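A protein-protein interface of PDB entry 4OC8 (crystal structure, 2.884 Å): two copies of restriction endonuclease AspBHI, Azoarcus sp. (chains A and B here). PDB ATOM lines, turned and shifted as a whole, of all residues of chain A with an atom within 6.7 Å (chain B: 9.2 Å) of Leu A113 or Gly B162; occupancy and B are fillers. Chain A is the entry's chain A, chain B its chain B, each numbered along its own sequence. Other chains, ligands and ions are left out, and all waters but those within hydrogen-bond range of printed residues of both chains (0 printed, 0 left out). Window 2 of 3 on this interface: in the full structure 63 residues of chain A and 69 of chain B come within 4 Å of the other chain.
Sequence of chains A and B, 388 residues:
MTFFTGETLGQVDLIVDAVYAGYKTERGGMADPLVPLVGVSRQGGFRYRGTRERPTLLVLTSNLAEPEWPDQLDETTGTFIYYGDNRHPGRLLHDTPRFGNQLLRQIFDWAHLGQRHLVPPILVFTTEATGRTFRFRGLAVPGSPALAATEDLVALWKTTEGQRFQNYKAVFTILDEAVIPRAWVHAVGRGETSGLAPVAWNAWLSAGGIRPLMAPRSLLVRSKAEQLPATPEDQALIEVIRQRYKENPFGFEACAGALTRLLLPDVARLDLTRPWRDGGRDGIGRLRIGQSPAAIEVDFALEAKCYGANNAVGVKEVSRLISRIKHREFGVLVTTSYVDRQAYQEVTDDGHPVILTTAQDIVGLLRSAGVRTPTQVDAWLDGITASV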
ATOM      1  N   GLN A 106     -38.064   3.782 -28.285  1.00  0.00           N
ATOM      2  CA  GLN A 106     -37.647   3.106 -29.507  1.00  0.00           C
ATOM      3  C   GLN A 106     -37.177   4.108 -30.563  1.00  0.00           C
ATOM      4  O   GLN A 106     -36.150   3.909 -31.202  1.00  0.00           O
ATOM      5  CB  GLN A 106     -38.786   2.234 -30.043  1.00  0.00           C
ATOM      6  CG  GLN A 106     -38.352   1.203 -31.068  1.00  0.00           C
ATOM      7  CD  GLN A 106     -37.189   0.342 -30.590  1.00  0.00           C
ATOM      8  OE1 GLN A 106     -36.070   0.447 -31.101  1.00  0.00           O
ATOM      9  NE2 GLN A 106     -37.453  -0.521 -29.612  1.00  0.00           N
ATOM     10  N   PHE A 108     -36.032   7.269 -30.061  1.00  0.00           N
ATOM     11  CA  PHE A 108     -34.744   7.852 -29.681  1.00  0.00           C
ATOM     12  C   PHE A 108     -33.604   6.839 -29.770  1.00  0.00           C
ATOM     13  O   PHE A 108     -32.459   7.198 -30.069  1.00  0.00           O
ATOM     14  CB  PHE A 108     -34.823   8.536 -28.313  1.00  0.00           C
ATOM     15  CG  PHE A 108     -35.500   9.872 -28.363  1.00  0.00           C
ATOM     16  CD1 PHE A 108     -36.879   9.971 -28.266  1.00  0.00           C
ATOM     17  CD2 PHE A 108     -34.760  11.029 -28.558  1.00  0.00           C
ATOM     18  CE1 PHE A 108     -37.508  11.200 -28.343  1.00  0.00           C
ATOM     19  CE2 PHE A 108     -35.383  12.259 -28.634  1.00  0.00           C
ATOM     20  CZ  PHE A 108     -36.758  12.345 -28.526  1.00  0.00           C
ATOM     21  N   ASP A 109     -33.937   5.572 -29.540  1.00  0.00           N
ATOM     22  CA  ASP A 109     -32.999   4.470 -29.734  1.00  0.00           C
ATOM     23  C   ASP A 109     -32.515   4.454 -31.177  1.00  0.00           C
ATOM     24  O   ASP A 109     -31.313   4.423 -31.436  1.00  0.00           O
ATOM     25  CB  ASP A 109     -33.656   3.126 -29.407  1.00  0.00           C
ATOM     26  CG  ASP A 109     -33.543   2.755 -27.942  1.00  0.00           C
ATOM     27  OD1 ASP A 109     -33.193   3.632 -27.120  1.00  0.00           O
ATOM     28  OD2 ASP A 109     -33.821   1.581 -27.611  1.00  0.00           O
ATOM     29  N   TRP A 110     -33.465   4.480 -32.109  1.00  0.00           N
ATOM     30  CA  TRP A 110     -33.158   4.447 -33.534  1.00  0.00           C
ATOM     31  C   TRP A 110     -32.337   5.657 -33.935  1.00  0.00           C
ATOM     32  O   TRP A 110     -31.275   5.518 -34.537  1.00  0.00           O
ATOM     33  CB  TRP A 110     -34.439   4.384 -34.365  1.00  0.00           C
ATOM     34  CG  TRP A 110     -35.114   3.059 -34.316  1.00  0.00           C
ATOM     35  CD1 TRP A 110     -34.520   1.843 -34.151  1.00  0.00           C
ATOM     36  CD2 TRP A 110     -36.522   2.811 -34.413  1.00  0.00           C
ATOM     37  NE1 TRP A 110     -35.470   0.851 -34.144  1.00  0.00           N
ATOM     38  CE2 TRP A 110     -36.706   1.419 -34.302  1.00  0.00           C
ATOM     39  CE3 TRP A 110     -37.641   3.629 -34.583  1.00  0.00           C
ATOM     40  CZ2 TRP A 110     -37.965   0.829 -34.368  1.00  0.00           C
ATOM     41  CZ3 TRP A 110     -38.890   3.040 -34.637  1.00  0.00           C
ATOM     42  CH2 TRP A 110     -39.043   1.654 -34.531  1.00  0.00           C
ATOM     43  N   ALA A 111     -32.833   6.842 -33.591  1.00  0.00           N
ATOM     44  CA  ALA A 111     -32.123   8.080 -33.879  1.00  0.00           C
ATOM     45  C   ALA A 111     -30.682   8.054 -33.370  1.00  0.00           C
ATOM     46  O   ALA A 111     -29.779   8.554 -34.035  1.00  0.00           O
ATOM     47  CB  ALA A 111     -32.869   9.259 -33.293  1.00  0.00           C
ATOM     48  N   HIS A 112     -30.463   7.454 -32.204  1.00  0.00           N
ATOM     49  CA  HIS A 112     -29.124   7.444 -31.617  1.00  0.00           C
ATOM     50  C   HIS A 112     -28.212   6.329 -32.114  1.00  0.00           C
ATOM     51  O   HIS A 112     -26.989   6.448 -32.041  1.00  0.00           O
ATOM     52  CB  HIS A 112     -29.198   7.443 -30.084  1.00  0.00           C
ATOM     53  CG  HIS A 112     -29.375   8.809 -29.503  1.00  0.00           C
ATOM     54  ND1 HIS A 112     -28.332   9.524 -28.963  1.00  0.00           N
ATOM     55  CD2 HIS A 112     -30.464   9.610 -29.434  1.00  0.00           C
ATOM     56  CE1 HIS A 112     -28.774  10.705 -28.561  1.00  0.00           C
ATOM     57  NE2 HIS A 112     -30.061  10.782 -28.838  1.00  0.00           N
ATOM     58  N   LEU A 113     -28.808   5.259 -32.629  1.00  0.00           N
ATOM     59  CA  LEU A 113     -28.052   4.082 -33.047  1.00  0.00           C
ATOM     60  C   LEU A 113     -27.632   4.102 -34.520  1.00  0.00           C
ATOM     61  O   LEU A 113     -26.976   3.177 -34.993  1.00  0.00           O
ATOM     62  CB  LEU A 113     -28.837   2.805 -32.734  1.00  0.00           C
ATOM     63  CG  LEU A 113     -28.780   2.393 -31.264  1.00  0.00           C
ATOM     64  CD1 LEU A 113     -29.901   1.430 -30.911  1.00  0.00           C
ATOM     65  CD2 LEU A 113     -27.421   1.786 -30.955  1.00  0.00           C
ATOM     66  N   GLY A 114     -28.001   5.155 -35.239  1.00  0.00           N
ATOM     67  CA  GLY A 114     -27.599   5.292 -36.627  1.00  0.00           C
ATOM     68  C   GLY A 114     -28.572   4.639 -37.594  1.00  0.00           C
ATOM     69  O   GLY A 114     -28.218   4.302 -38.718  1.00  0.00           O
ATOM     70  N   GLN A 115     -29.803   4.451 -37.136  1.00  0.00           N
ATOM     71  CA  GLN A 115     -30.862   3.900 -37.955  1.00  0.00           C
ATOM     72  C   GLN A 115     -32.027   4.869 -38.034  1.00  0.00           C
ATOM     73  O   GLN A 115     -33.067   4.633 -37.421  1.00  0.00           O
ATOM     74  CB  GLN A 115     -31.384   2.606 -37.359  1.00  0.00           C
ATOM     75  CG  GLN A 115     -30.334   1.649 -36.867  1.00  0.00           C
ATOM     76  CD  GLN A 115     -30.940   0.567 -36.013  1.00  0.00           C
ATOM     77  OE1 GLN A 115     -31.800   0.834 -35.173  1.00  0.00           O
ATOM     78  NE2 GLN A 115     -30.514  -0.665 -36.233  1.00  0.00           N
ATOM     79  N   ARG A 116     -31.872   5.936 -38.810  1.00  0.00           N
ATOM     80  CA  ARG A 116     -32.894   6.971 -38.878  1.00  0.00           C
ATOM     81  C   ARG A 116     -34.013   6.657 -39.858  1.00  0.00           C
ATOM     82  O   ARG A 116     -35.038   7.344 -39.882  1.00  0.00           O
ATOM     83  CB  ARG A 116     -32.265   8.314 -39.220  1.00  0.00           C
ATOM     84  CG  ARG A 116     -31.375   8.856 -38.129  1.00  0.00           C
ATOM     85  CD  ARG A 116     -30.801  10.190 -38.531  1.00  0.00           C
ATOM     86  NE  ARG A 116     -29.857  10.052 -39.632  1.00  0.00           N
ATOM     87  CZ  ARG A 116     -28.538  10.054 -39.482  1.00  0.00           C
ATOM     88  NH1 ARG A 116     -28.008  10.199 -38.273  1.00  0.00           N
ATOM     89  NH2 ARG A 116     -27.750   9.926 -40.541  1.00  0.00           N
ATOM     90  N   PRO B  89     -23.470  -1.180 -20.611  1.00  0.00           N
ATOM     91  CA  PRO B  89     -24.784  -1.726 -21.000  1.00  0.00           C
ATOM     92  C   PRO B  89     -25.024  -3.141 -20.484  1.00  0.00           C
ATOM     93  O   PRO B  89     -24.056  -3.832 -20.161  1.00  0.00           O
ATOM     94  CB  PRO B  89     -24.712  -1.747 -22.536  1.00  0.00           C
ATOM     95  CG  PRO B  89     -23.268  -1.853 -22.862  1.00  0.00           C
ATOM     96  CD  PRO B  89     -22.532  -1.110 -21.751  1.00  0.00           C
ATOM     97  N   TRP B 157     -30.143   8.238 -21.178  1.00  0.00           N
ATOM     98  CA  TRP B 157     -29.784   7.124 -22.043  1.00  0.00           C
ATOM     99  C   TRP B 157     -28.389   7.379 -22.613  1.00  0.00           C
ATOM    100  O   TRP B 157     -28.129   8.428 -23.205  1.00  0.00           O
ATOM    101  CB  TRP B 157     -30.795   6.956 -23.181  1.00  0.00           C
ATOM    102  CG  TRP B 157     -32.088   6.271 -22.819  1.00  0.00           C
ATOM    103  CD1 TRP B 157     -33.325   6.849 -22.722  1.00  0.00           C
ATOM    104  CD2 TRP B 157     -32.277   4.878 -22.531  1.00  0.00           C
ATOM    105  NE1 TRP B 157     -34.266   5.903 -22.382  1.00  0.00           N
ATOM    106  CE2 TRP B 157     -33.648   4.686 -22.257  1.00  0.00           C
ATOM    107  CE3 TRP B 157     -31.418   3.775 -22.469  1.00  0.00           C
ATOM    108  CZ2 TRP B 157     -34.179   3.442 -21.932  1.00  0.00           C
ATOM    109  CZ3 TRP B 157     -31.946   2.539 -22.141  1.00  0.00           C
ATOM    110  CH2 TRP B 157     -33.314   2.383 -21.876  1.00  0.00           C
ATOM    111  N   LYS B 158     -27.490   6.424 -22.417  1.00  0.00           N
ATOM    112  CA  LYS B 158     -26.162   6.482 -23.005  1.00  0.00           C
ATOM    113  C   LYS B 158     -26.035   5.374 -24.054  1.00  0.00           C
ATOM    114  O   LYS B 158     -26.607   4.279 -23.897  1.00  0.00           O
ATOM    115  CB  LYS B 158     -25.093   6.328 -21.923  1.00  0.00           C
ATOM    116  CG  LYS B 158     -23.670   6.533 -22.408  1.00  0.00           C
ATOM    117  CD  LYS B 158     -23.401   7.992 -22.738  1.00  0.00           C
ATOM    118  CE  LYS B 158     -22.115   8.157 -23.546  1.00  0.00           C
ATOM    119  NZ  LYS B 158     -22.241   7.656 -24.955  1.00  0.00           N
ATOM    120  N   THR B 159     -25.296   5.672 -25.122  1.00  0.00           N
ATOM    121  CA  THR B 159     -25.100   4.740 -26.231  1.00  0.00           C
ATOM    122  C   THR B 159     -23.670   4.217 -26.293  1.00  0.00           C
ATOM    123  O   THR B 159     -22.722   4.990 -26.438  1.00  0.00           O
ATOM    124  CB  THR B 159     -25.407   5.403 -27.580  1.00  0.00           C
ATOM    125  OG1 THR B 159     -26.773   5.842 -27.609  1.00  0.00           O
ATOM    126  CG2 THR B 159     -25.154   4.433 -28.713  1.00  0.00           C
ATOM    127  N   THR B 160     -23.524   2.901 -26.191  1.00  0.00           N
ATOM    128  CA  THR B 160     -22.213   2.267 -26.245  1.00  0.00           C
ATOM    129  C   THR B 160     -22.232   0.966 -27.046  1.00  0.00           C
ATOM    130  O   THR B 160     -22.989   0.043 -26.729  1.00  0.00           O
ATOM    131  CB  THR B 160     -21.661   1.998 -24.836  1.00  0.00           C
ATOM    132  OG1 THR B 160     -21.180   3.226 -24.278  1.00  0.00           O
ATOM    133  CG2 THR B 160     -20.522   0.990 -24.888  1.00  0.00           C
ATOM    134  N   GLU B 161     -21.399   0.920 -28.088  1.00  0.00           N
ATOM    135  CA  GLU B 161     -21.207  -0.267 -28.919  1.00  0.00           C
ATOM    136  C   GLU B 161     -22.515  -0.863 -29.428  1.00  0.00           C
ATOM    137  O   GLU B 161     -22.704  -2.079 -29.399  1.00  0.00           O
ATOM    138  CB  GLU B 161     -20.402  -1.336 -28.170  1.00  0.00           C
ATOM    139  CG  GLU B 161     -18.957  -0.948 -27.865  1.00  0.00           C
ATOM    140  CD  GLU B 161     -18.045  -1.039 -29.079  1.00  0.00           C
ATOM    141  OE1 GLU B 161     -18.472  -1.600 -30.108  1.00  0.00           O
ATOM    142  OE2 GLU B 161     -16.897  -0.549 -28.999  1.00  0.00           O
ATOM    143  N   GLY B 162     -23.416  -0.002 -29.881  1.00  0.00           N
ATOM    144  CA  GLY B 162     -24.661  -0.452 -30.474  1.00  0.00           C
ATOM    145  C   GLY B 162     -25.750  -0.787 -29.473  1.00  0.00           C
ATOM    146  O   GLY B 162     -26.842  -1.202 -29.860  1.00  0.00           O
ATOM    147  N   GLN B 163     -25.456  -0.605 -28.187  1.00  0.00           N
ATOM    148  CA  GLN B 163     -26.439  -0.840 -27.134  1.00  0.00           C
ATOM    149  C   GLN B 163     -26.779   0.447 -26.393  1.00  0.00           C
ATOM    150  O   GLN B 163     -26.002   1.401 -26.400  1.00  0.00           O
ATOM    151  CB  GLN B 163     -25.923  -1.879 -26.152  1.00  0.00           C
ATOM    152  CG  GLN B 163     -25.543  -3.191 -26.798  1.00  0.00           C
ATOM    153  CD  GLN B 163     -24.981  -4.172 -25.799  1.00  0.00           C
ATOM    154  OE1 GLN B 163     -23.771  -4.385 -25.736  1.00  0.00           O
ATOM    155  NE2 GLN B 163     -25.859  -4.773 -25.003  1.00  0.00           N
ATOM    156  N   ARG B 164     -27.946   0.472 -25.756  1.00  0.00           N
ATOM    157  CA  ARG B 164     -28.395   1.660 -25.035  1.00  0.00           C
ATOM    158  C   ARG B 164     -28.776   1.352 -23.592  1.00  0.00           C
ATOM    159  O   ARG B 164     -29.610   0.483 -23.336  1.00  0.00           O
ATOM    160  CB  ARG B 164     -29.582   2.308 -25.750  1.00  0.00           C
ATOM    161  CG  ARG B 164     -29.245   2.874 -27.116  1.00  0.00           C
ATOM    162  CD  ARG B 164     -30.154   4.039 -27.443  1.00  0.00           C
ATOM    163  NE  ARG B 164     -29.632   5.304 -26.938  1.00  0.00           N
ATOM    164  CZ  ARG B 164     -30.389   6.341 -26.599  1.00  0.00           C
ATOM    165  NH1 ARG B 164     -31.710   6.259 -26.690  1.00  0.00           N
ATOM    166  NH2 ARG B 164     -29.825   7.459 -26.160  1.00  0.00           N
ATOM    167  N   PHE B 165     -28.174   2.073 -22.651  1.00  0.00           N
ATOM    168  CA  PHE B 165     -28.460   1.830 -21.236  1.00  0.00           C
ATOM    169  C   PHE B 165     -28.770   3.113 -20.466  1.00  0.00           C
ATOM    170  O   PHE B 165     -28.451   4.212 -20.915  1.00  0.00           O
ATOM    171  CB  PHE B 165     -27.310   1.065 -20.569  1.00  0.00           C
ATOM    172  CG  PHE B 165     -25.994   1.796 -20.584  1.00  0.00           C
ATOM    173  CD1 PHE B 165     -25.225   1.850 -21.737  1.00  0.00           C
ATOM    174  CD2 PHE B 165     -25.521   2.421 -19.439  1.00  0.00           C
ATOM    175  CE1 PHE B 165     -24.015   2.522 -21.750  1.00  0.00           C
ATOM    176  CE2 PHE B 165     -24.308   3.091 -19.445  1.00  0.00           C
ATOM    177  CZ  PHE B 165     -23.556   3.140 -20.600  1.00  0.00           C
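No position is printed for both chains. Of the 5 pairs that touch across the chains among the printed residues, none has its exchanged pair printed and touching as well.
Phe A108 touches Arg B164 (O to NH1, 3.6 Å). His A112 touches Thr B159 (CB to OG1, 3.8 Å). His A112 touches Arg B164. Leu A113 touches Gly B162 (CD2 to O, 3.2 Å).
Gly B162 touches one residue of chain A. Of the printed residues of chain B, Asp A109 touches Arg B164. Printed residues of chain A within 4 Å of Thr B159: His A112. Printed residues of chain B within 4 Å of His A112: Thr B159 (3.8 Å) and Arg B164 (3.6 Å). Of the printed residues of chain A, Arg B164 touches Phe A108 (3.6 Å), Asp A109 (3.0 Å) and His A112 (3.6 Å). Printed residues of chain B within 4 Å of Phe A108: Arg B164. The nearest residue of chain B that does not touch Leu A113 is Arg B164 (4.1 Å). The nearest printed residue of chain A that does not touch Gly B162 is Asp A109 (7.4 Å).
Of the 10 printed residues of chain A, 4 touch a printed residue of chain B. Hydrophobic or aromatic side chains of chain A within 4 Å of the printed part of chain B: His A112 and Leu A113. Printed residues of chain B that touch a printed residue of chain A: Thr B159, Gly B162 and Arg B164.
OD1 of Asp A109 lies within salt-bridge range of NH1 of Arg B164 (3.0 Å).
The side-chain hydroxyl (OG1) of Thr B159 lies within hydrogen-bond range of the guanidinium group (NE) of Arg B164.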
